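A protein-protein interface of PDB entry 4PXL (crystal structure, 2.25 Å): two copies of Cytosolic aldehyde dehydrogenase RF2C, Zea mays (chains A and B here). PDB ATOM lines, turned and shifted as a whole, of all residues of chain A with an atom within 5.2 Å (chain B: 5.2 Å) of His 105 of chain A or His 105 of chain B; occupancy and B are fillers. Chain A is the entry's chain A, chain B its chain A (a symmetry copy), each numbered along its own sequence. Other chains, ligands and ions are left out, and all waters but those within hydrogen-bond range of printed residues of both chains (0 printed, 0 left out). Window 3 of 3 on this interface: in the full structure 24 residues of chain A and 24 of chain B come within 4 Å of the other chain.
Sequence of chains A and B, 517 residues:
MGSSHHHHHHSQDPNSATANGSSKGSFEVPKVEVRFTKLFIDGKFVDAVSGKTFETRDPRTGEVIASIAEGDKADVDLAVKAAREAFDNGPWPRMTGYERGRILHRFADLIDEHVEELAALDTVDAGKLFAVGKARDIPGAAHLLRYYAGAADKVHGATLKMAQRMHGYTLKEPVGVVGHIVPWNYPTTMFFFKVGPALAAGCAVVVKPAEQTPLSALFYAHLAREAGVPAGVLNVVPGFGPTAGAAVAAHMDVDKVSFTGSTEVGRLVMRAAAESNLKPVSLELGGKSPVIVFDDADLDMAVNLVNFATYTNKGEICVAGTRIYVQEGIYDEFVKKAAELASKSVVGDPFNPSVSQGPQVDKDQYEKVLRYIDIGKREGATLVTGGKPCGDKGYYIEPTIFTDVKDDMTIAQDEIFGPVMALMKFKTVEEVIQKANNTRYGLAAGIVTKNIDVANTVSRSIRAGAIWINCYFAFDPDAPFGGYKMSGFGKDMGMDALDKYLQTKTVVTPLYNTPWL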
ATOM      1  N   ARG A 100      -0.802  29.389 -20.452  1.00  0.00           N
ATOM      2  CA  ARG A 100       0.420  30.191 -20.676  1.00  0.00           C
ATOM      3  C   ARG A 100       1.319  29.411 -21.660  1.00  0.00           C
ATOM      4  O   ARG A 100       1.841  30.009 -22.598  1.00  0.00           O
ATOM      5  CB  ARG A 100       1.172  30.482 -19.363  1.00  0.00           C
ATOM      6  CG  ARG A 100       0.573  31.647 -18.547  1.00  0.00           C
ATOM      7  CD  ARG A 100       1.490  32.028 -17.400  1.00  0.00           C
ATOM      8  NE  ARG A 100       1.655  30.936 -16.432  1.00  0.00           N
ATOM      9  CZ  ARG A 100       0.830  30.730 -15.415  1.00  0.00           C
ATOM     10  NH1 ARG A 100      -0.178  31.567 -15.191  1.00  0.00           N
ATOM     11  NH2 ARG A 100       1.006  29.693 -14.611  1.00  0.00           N
ATOM     12  N   GLY A 101       1.382  28.080 -21.493  1.00  0.00           N
ATOM     13  CA  GLY A 101       2.128  27.160 -22.355  1.00  0.00           C
ATOM     14  C   GLY A 101       1.653  27.190 -23.786  1.00  0.00           C
ATOM     15  O   GLY A 101       2.464  27.199 -24.700  1.00  0.00           O
ATOM     16  N   ARG A 102       0.337  27.254 -24.005  1.00  0.00           N
ATOM     17  CA  ARG A 102      -0.238  27.295 -25.355  1.00  0.00           C
ATOM     18  C   ARG A 102       0.188  28.572 -26.072  1.00  0.00           C
ATOM     19  O   ARG A 102       0.520  28.522 -27.258  1.00  0.00           O
ATOM     20  CB  ARG A 102      -1.780  27.162 -25.312  1.00  0.00           C
ATOM     21  CG  ARG A 102      -2.234  25.772 -24.870  1.00  0.00           C
ATOM     22  CD  ARG A 102      -2.361  24.811 -26.030  1.00  0.00           C
ATOM     23  NE  ARG A 102      -3.718  24.833 -26.562  1.00  0.00           N
ATOM     24  CZ  ARG A 102      -4.054  24.519 -27.808  1.00  0.00           C
ATOM     25  NH1 ARG A 102      -5.325  24.559 -28.187  1.00  0.00           N
ATOM     26  NH2 ARG A 102      -3.119  24.185 -28.693  1.00  0.00           N
ATOM     27  N   ILE A 103       0.236  29.699 -25.334  1.00  0.00           N
ATOM     28  CA  ILE A 103       0.658  30.989 -25.873  1.00  0.00           C
ATOM     29  C   ILE A 103       2.163  30.943 -26.176  1.00  0.00           C
ATOM     30  O   ILE A 103       2.590  31.359 -27.256  1.00  0.00           O
ATOM     31  CB  ILE A 103       0.235  32.136 -24.924  1.00  0.00           C
ATOM     32  CG1 ILE A 103      -1.309  32.360 -25.029  1.00  0.00           C
ATOM     33  CG2 ILE A 103       1.057  33.435 -25.180  1.00  0.00           C
ATOM     34  CD1 ILE A 103      -1.992  33.263 -23.899  1.00  0.00           C
ATOM     35  N   LEU A 104       2.951  30.340 -25.275  1.00  0.00           N
ATOM     36  CA  LEU A 104       4.382  30.226 -25.519  1.00  0.00           C
ATOM     37  C   LEU A 104       4.700  29.291 -26.685  1.00  0.00           C
ATOM     38  O   LEU A 104       5.691  29.496 -27.365  1.00  0.00           O
ATOM     39  CB  LEU A 104       5.151  29.838 -24.247  1.00  0.00           C
ATOM     40  CG  LEU A 104       5.057  30.781 -23.057  1.00  0.00           C
ATOM     41  CD1 LEU A 104       5.902  30.260 -21.912  1.00  0.00           C
ATOM     42  CD2 LEU A 104       5.433  32.233 -23.421  1.00  0.00           C
ATOM     43  N   HIS A 105       3.860  28.276 -26.918  1.00  0.00           N
ATOM     44  CA  HIS A 105       4.019  27.355 -28.040  1.00  0.00           C
ATOM     45  C   HIS A 105       3.759  28.073 -29.380  1.00  0.00           C
ATOM     46  O   HIS A 105       4.401  27.766 -30.383  1.00  0.00           O
ATOM     47  CB  HIS A 105       3.099  26.135 -27.870  1.00  0.00           C
ATOM     48  CG  HIS A 105       3.861  24.986 -27.334  1.00  0.00           C
ATOM     49  ND1 HIS A 105       4.809  24.372 -28.141  1.00  0.00           N
ATOM     50  CD2 HIS A 105       3.855  24.372 -26.131  1.00  0.00           C
ATOM     51  CE1 HIS A 105       5.354  23.425 -27.406  1.00  0.00           C
ATOM     52  NE2 HIS A 105       4.826  23.379 -26.196  1.00  0.00           N
ATOM     53  N   ARG A 106       2.843  29.038 -29.362  1.00  0.00           N
ATOM     54  CA  ARG A 106       2.451  29.833 -30.509  1.00  0.00           C
ATOM     55  C   ARG A 106       3.573  30.801 -30.821  1.00  0.00           C
ATOM     56  O   ARG A 106       3.920  31.011 -31.996  1.00  0.00           O
ATOM     57  CB  ARG A 106       1.166  30.624 -30.172  1.00  0.00           C
ATOM     58  CG  ARG A 106       0.346  31.049 -31.388  1.00  0.00           C
ATOM     59  CD  ARG A 106      -1.044  31.533 -30.971  1.00  0.00           C
ATOM     60  NE  ARG A 106      -1.843  30.486 -30.311  1.00  0.00           N
ATOM     61  CZ  ARG A 106      -2.495  30.642 -29.159  1.00  0.00           C
ATOM     62  NH1 ARG A 106      -3.187  29.633 -28.639  1.00  0.00           N
ATOM     63  NH2 ARG A 106      -2.462  31.813 -28.518  1.00  0.00           N
ATOM     64  N   PHE A 107       4.157  31.357 -29.731  1.00  0.00           N
ATOM     65  CA  PHE A 107       5.273  32.269 -29.767  1.00  0.00           C
ATOM     66  C   PHE A 107       6.490  31.552 -30.405  1.00  0.00           C
ATOM     67  O   PHE A 107       7.098  32.107 -31.326  1.00  0.00           O
ATOM     68  CB  PHE A 107       5.539  32.839 -28.353  1.00  0.00           C
ATOM     69  CG  PHE A 107       6.572  33.935 -28.189  1.00  0.00           C
ATOM     70  CD1 PHE A 107       7.197  34.509 -29.297  1.00  0.00           C
ATOM     71  CD2 PHE A 107       6.950  34.364 -26.927  1.00  0.00           C
ATOM     72  CE1 PHE A 107       8.164  35.503 -29.135  1.00  0.00           C
ATOM     73  CE2 PHE A 107       7.922  35.349 -26.768  1.00  0.00           C
ATOM     74  CZ  PHE A 107       8.519  35.913 -27.869  1.00  0.00           C
ATOM     75  N   ALA A 108       6.769  30.307 -29.983  1.00  0.00           N
ATOM     76  CA  ALA A 108       7.849  29.487 -30.542  1.00  0.00           C
ATOM     77  C   ALA A 108       7.605  29.209 -32.051  1.00  0.00           C
ATOM     78  O   ALA A 108       8.529  29.321 -32.847  1.00  0.00           O
ATOM     79  CB  ALA A 108       7.970  28.190 -29.774  1.00  0.00           C
ATOM     80  N   ASP A 109       6.375  28.887 -32.439  1.00  0.00           N
ATOM     81  CA  ASP A 109       6.028  28.654 -33.852  1.00  0.00           C
ATOM     82  C   ASP A 109       6.296  29.887 -34.708  1.00  0.00           C
ATOM     83  O   ASP A 109       6.850  29.757 -35.792  1.00  0.00           O
ATOM     84  CB  ASP A 109       4.562  28.178 -34.002  1.00  0.00           C
ATOM     85  CG  ASP A 109       4.306  26.769 -33.471  1.00  0.00           C
ATOM     86  OD1 ASP A 109       5.249  25.952 -33.466  1.00  0.00           O
ATOM     87  OD2 ASP A 109       3.163  26.486 -33.056  1.00  0.00           O
ATOM     88  N   ARG A 146       9.796  26.119 -26.214  1.00  0.00           N
ATOM     89  CA  ARG A 146       8.904  24.956 -26.188  1.00  0.00           C
ATOM     90  C   ARG A 146       9.148  24.141 -24.943  1.00  0.00           C
ATOM     91  O   ARG A 146       8.188  23.657 -24.348  1.00  0.00           O
ATOM     92  CB  ARG A 146       9.089  24.071 -27.418  1.00  0.00           C
ATOM     93  CG  ARG A 146       8.495  24.686 -28.653  1.00  0.00           C
ATOM     94  CD  ARG A 146       8.596  23.756 -29.842  1.00  0.00           C
ATOM     95  NE  ARG A 146       8.023  24.429 -30.997  1.00  0.00           N
ATOM     96  CZ  ARG A 146       8.730  24.981 -31.976  1.00  0.00           C
ATOM     97  NH1 ARG A 146       8.121  25.619 -32.958  1.00  0.00           N
ATOM     98  NH2 ARG A 146      10.054  24.873 -31.993  1.00  0.00           N
ATOM     99  N   ALA A 149       7.357  26.091 -22.230  1.00  0.00           N
ATOM    100  CA  ALA A 149       5.927  26.002 -22.496  1.00  0.00           C
ATOM    101  C   ALA A 149       5.414  24.636 -21.973  1.00  0.00           C
ATOM    102  O   ALA A 149       4.396  24.597 -21.293  1.00  0.00           O
ATOM    103  CB  ALA A 149       5.661  26.142 -23.995  1.00  0.00           C
ATOM    104  N   GLY A 150       6.173  23.568 -22.213  1.00  0.00           N
ATOM    105  CA  GLY A 150       5.845  22.217 -21.760  1.00  0.00           C
ATOM    106  C   GLY A 150       5.997  22.000 -20.264  1.00  0.00           C
ATOM    107  O   GLY A 150       5.425  21.052 -19.724  1.00  0.00           O
ATOM    108  N   ARG B 100       9.891  13.302 -30.059  1.00  0.00           N
ATOM    109  CA  ARG B 100       8.670  12.499 -29.835  1.00  0.00           C
ATOM    110  C   ARG B 100       7.540  13.470 -29.428  1.00  0.00           C
ATOM    111  O   ARG B 100       6.433  13.356 -29.949  1.00  0.00           O
ATOM    112  CB  ARG B 100       8.875  11.417 -28.757  1.00  0.00           C
ATOM    113  CG  ARG B 100       9.594  10.154 -29.273  1.00  0.00           C
ATOM    114  CD  ARG B 100       9.553   9.048 -28.234  1.00  0.00           C
ATOM    115  NE  ARG B 100      10.268   9.413 -27.004  1.00  0.00           N
ATOM    116  CZ  ARG B 100      11.569   9.226 -26.833  1.00  0.00           C
ATOM    117  NH1 ARG B 100      12.288   8.627 -27.775  1.00  0.00           N
ATOM    118  NH2 ARG B 100      12.160   9.628 -25.718  1.00  0.00           N
ATOM    119  N   GLY B 101       7.876  14.471 -28.597  1.00  0.00           N
ATOM    120  CA  GLY B 101       6.966  15.526 -28.143  1.00  0.00           C
ATOM    121  C   GLY B 101       6.412  16.347 -29.281  1.00  0.00           C
ATOM    122  O   GLY B 101       5.228  16.647 -29.300  1.00  0.00           O
ATOM    123  N   ARG B 102       7.245  16.682 -30.270  1.00  0.00           N
ATOM    124  CA  ARG B 102       6.815  17.472 -31.430  1.00  0.00           C
ATOM    125  C   ARG B 102       5.778  16.701 -32.239  1.00  0.00           C
ATOM    126  O   ARG B 102       4.792  17.291 -32.686  1.00  0.00           O
ATOM    127  CB  ARG B 102       8.022  17.882 -32.309  1.00  0.00           C
ATOM    128  CG  ARG B 102       8.931  18.896 -31.617  1.00  0.00           C
ATOM    129  CD  ARG B 102       8.495  20.323 -31.863  1.00  0.00           C
ATOM    130  NE  ARG B 102       9.169  20.866 -33.036  1.00  0.00           N
ATOM    131  CZ  ARG B 102       8.700  21.845 -33.801  1.00  0.00           C
ATOM    132  NH1 ARG B 102       9.402  22.274 -34.841  1.00  0.00           N
ATOM    133  NH2 ARG B 102       7.512  22.387 -33.546  1.00  0.00           N
ATOM    134  N   ILE B 103       5.972  15.373 -32.372  1.00  0.00           N
ATOM    135  CA  ILE B 103       5.047  14.498 -33.088  1.00  0.00           C
ATOM    136  C   ILE B 103       3.740  14.380 -32.289  1.00  0.00           C
ATOM    137  O   ILE B 103       2.654  14.510 -32.858  1.00  0.00           O
ATOM    138  CB  ILE B 103       5.723  13.143 -33.407  1.00  0.00           C
ATOM    139  CG1 ILE B 103       6.763  13.335 -34.558  1.00  0.00           C
ATOM    140  CG2 ILE B 103       4.676  12.030 -33.714  1.00  0.00           C
ATOM    141  CD1 ILE B 103       7.799  12.141 -34.810  1.00  0.00           C
ATOM    142  N   LEU B 104       3.847  14.245 -30.960  1.00  0.00           N
ATOM    143  CA  LEU B 104       2.646  14.168 -30.139  1.00  0.00           C
ATOM    144  C   LEU B 104       1.868  15.483 -30.121  1.00  0.00           C
ATOM    145  O   LEU B 104       0.657  15.461 -29.994  1.00  0.00           O
ATOM    146  CB  LEU B 104       2.955  13.666 -28.720  1.00  0.00           C
ATOM    147  CG  LEU B 104       3.579  12.284 -28.587  1.00  0.00           C
ATOM    148  CD1 LEU B 104       3.778  11.943 -27.124  1.00  0.00           C
ATOM    149  CD2 LEU B 104       2.765  11.195 -29.316  1.00  0.00           C
ATOM    150  N   HIS B 105       2.561  16.619 -30.256  1.00  0.00           N
ATOM    151  CA  HIS B 105       1.927  17.933 -30.321  1.00  0.00           C
ATOM    152  C   HIS B 105       1.126  18.092 -31.629  1.00  0.00           C
ATOM    153  O   HIS B 105       0.078  18.735 -31.641  1.00  0.00           O
ATOM    154  CB  HIS B 105       2.977  19.047 -30.167  1.00  0.00           C
ATOM    155  CG  HIS B 105       2.985  19.559 -28.780  1.00  0.00           C
ATOM    156  ND1 HIS B 105       1.896  20.289 -28.325  1.00  0.00           N
ATOM    157  CD2 HIS B 105       3.877  19.441 -27.772  1.00  0.00           C
ATOM    158  CE1 HIS B 105       2.150  20.577 -27.065  1.00  0.00           C
ATOM    159  NE2 HIS B 105       3.317  20.094 -26.679  1.00  0.00           N
ATOM    160  N   ARG B 106       1.621  17.476 -32.699  1.00  0.00           N
ATOM    161  CA  ARG B 106       1.025  17.497 -34.021  1.00  0.00           C
ATOM    162  C   ARG B 106      -0.213  16.625 -33.997  1.00  0.00           C
ATOM    163  O   ARG B 106      -1.257  16.990 -34.563  1.00  0.00           O
ATOM    164  CB  ARG B 106       2.033  16.935 -35.049  1.00  0.00           C
ATOM    165  CG  ARG B 106       1.790  17.389 -36.487  1.00  0.00           C
ATOM    166  CD  ARG B 106       2.991  17.061 -37.377  1.00  0.00           C
ATOM    167  NE  ARG B 106       4.223  17.750 -36.956  1.00  0.00           N
ATOM    168  CZ  ARG B 106       5.404  17.156 -36.786  1.00  0.00           C
ATOM    169  NH1 ARG B 106       6.460  17.865 -36.397  1.00  0.00           N
ATOM    170  NH2 ARG B 106       5.539  15.846 -37.006  1.00  0.00           N
ATOM    171  N   PHE B 107      -0.078  15.474 -33.291  1.00  0.00           N
ATOM    172  CA  PHE B 107      -1.125  14.505 -33.084  1.00  0.00           C
ATOM    173  C   PHE B 107      -2.288  15.178 -32.309  1.00  0.00           C
ATOM    174  O   PHE B 107      -3.438  15.071 -32.745  1.00  0.00           O
ATOM    175  CB  PHE B 107      -0.551  13.242 -32.400  1.00  0.00           C
ATOM    176  CG  PHE B 107      -1.448  12.034 -32.226  1.00  0.00           C
ATOM    177  CD1 PHE B 107      -2.734  12.006 -32.768  1.00  0.00           C
ATOM    178  CD2 PHE B 107      -1.025  10.942 -31.485  1.00  0.00           C
ATOM    179  CE1 PHE B 107      -3.562  10.897 -32.584  1.00  0.00           C
ATOM    180  CE2 PHE B 107      -1.856   9.841 -31.294  1.00  0.00           C
ATOM    181  CZ  PHE B 107      -3.114   9.823 -31.845  1.00  0.00           C
ATOM    182  N   ALA B 108      -1.970  15.929 -31.242  1.00  0.00           N
ATOM    183  CA  ALA B 108      -2.959  16.674 -30.455  1.00  0.00           C
ATOM    184  C   ALA B 108      -3.669  17.741 -31.331  1.00  0.00           C
ATOM    185  O   ALA B 108      -4.886  17.871 -31.265  1.00  0.00           O
ATOM    186  CB  ALA B 108      -2.294  17.322 -29.261  1.00  0.00           C
ATOM    187  N   ASP B 109      -2.928  18.467 -32.162  1.00  0.00           N
ATOM    188  CA  ASP B 109      -3.511  19.469 -33.072  1.00  0.00           C
ATOM    189  C   ASP B 109      -4.508  18.838 -34.038  1.00  0.00           C
ATOM    190  O   ASP B 109      -5.579  19.395 -34.244  1.00  0.00           O
ATOM    191  CB  ASP B 109      -2.410  20.246 -33.835  1.00  0.00           C
ATOM    192  CG  ASP B 109      -1.590  21.190 -32.956  1.00  0.00           C
ATOM    193  OD1 ASP B 109      -2.122  21.666 -31.933  1.00  0.00           O
ATOM    194  OD2 ASP B 109      -0.415  21.446 -33.291  1.00  0.00           O
ATOM    195  N   ARG B 146      -0.981  16.798 -24.983  1.00  0.00           N
ATOM    196  CA  ARG B 146      -0.055  17.934 -24.925  1.00  0.00           C
ATOM    197  C   ARG B 146       0.718  17.909 -23.630  1.00  0.00           C
ATOM    198  O   ARG B 146       1.911  18.199 -23.641  1.00  0.00           O
ATOM    199  CB  ARG B 146      -0.785  19.269 -25.054  1.00  0.00           C
ATOM    200  CG  ARG B 146      -1.248  19.527 -26.459  1.00  0.00           C
ATOM    201  CD  ARG B 146      -1.879  20.896 -26.594  1.00  0.00           C
ATOM    202  NE  ARG B 146      -2.320  21.060 -27.971  1.00  0.00           N
ATOM    203  CZ  ARG B 146      -3.580  20.967 -28.375  1.00  0.00           C
ATOM    204  NH1 ARG B 146      -3.878  21.077 -29.656  1.00  0.00           N
ATOM    205  NH2 ARG B 146      -4.558  20.788 -27.493  1.00  0.00           N
ATOM    206  N   ALA B 149       3.360  15.254 -24.216  1.00  0.00           N
ATOM    207  CA  ALA B 149       4.280  15.765 -25.225  1.00  0.00           C
ATOM    208  C   ALA B 149       5.278  16.730 -24.536  1.00  0.00           C
ATOM    209  O   ALA B 149       6.477  16.620 -24.766  1.00  0.00           O
ATOM    210  CB  ALA B 149       3.504  16.486 -26.327  1.00  0.00           C
ATOM    211  N   GLY B 150       4.782  17.580 -23.638  1.00  0.00           N
ATOM    212  CA  GLY B 150       5.595  18.531 -22.880  1.00  0.00           C
ATOM    213  C   GLY B 150       6.470  17.899 -21.811  1.00  0.00           C
ATOM    214  O   GLY B 150       7.436  18.521 -21.367  1.00  0.00           O
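OD1 of Asp 109 of chain A lies within salt-bridge range of NH1 of Arg 146 of chain A (2.9 Å).
The side-chain carboxylate of Asp 109 of chain B lies within salt-bridge range of the guanidinium group of Arg 146 of chain B (2.9 Å).
NE2 of His 105 of chain A touches NE2 of His 105 of chain B, 3.6 Å away.
O of Gly 150 of chain A touches O of Gly 150 of chain B (3.6 Å).
The guanidinium group (NE) of Arg 146 of chain B sits close to the guanidinium group (NH2) of Arg 102 of chain A (3.3 Å).
The guanidinium group of Arg 146 of chain A lies close to the guanidinium group of Arg 102 of chain B, at 3.3 Å.
Of the printed residues of chain A, Gly 150 of chain B touches Gly 150 (3.6 Å).
Of the printed residues of chain B, Arg 102 of chain A touches Arg 146.
Of the printed residues of chain A, Arg 146 of chain B touches Arg 102 (3.3 Å).
Printed residues of chain B within 4 Å of Arg 146 of chain A: Arg 102.
Phe 107 of chain A touches none of the printed residues of chain B.
Ile 103 of chain B touches none of the printed residues of chain A.
The nearest printed residue of chain B that does not touch His 105 of chain A is Gly 150 of chain B (5.9 Å).
The nearest printed residue of chain B that does not touch Arg 102 of chain A is Asp 109 of chain B (4.2 Å).
Of the 13 printed residues of chain B, 4 touch a printed residue of chain A.
Printed residues of chain A that touch a printed residue of chain B: Arg 102, His 105, Arg 146 and Gly 150.
Among the printed residues, 4 pairs touch across the chains.
Among the printed residues, no Asp or Glu carboxylate lies within 4 Å of a Lys or Arg side-chain nitrogen of the other chain.
Arg 102 of chain A touches Arg 146 of chain B, and with the chains exchanged Arg 146 of chain A touches Arg 102 of chain B.
His 105 of chain A touches its own counterpart, His 105 of chain B.
Gly 150 of chain B touches its own counterpart, Gly 150 of chain A.
Of the 4 pairs that touch across the chains among the printed residues, 4 have their exchanged pair printed and touching as well.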
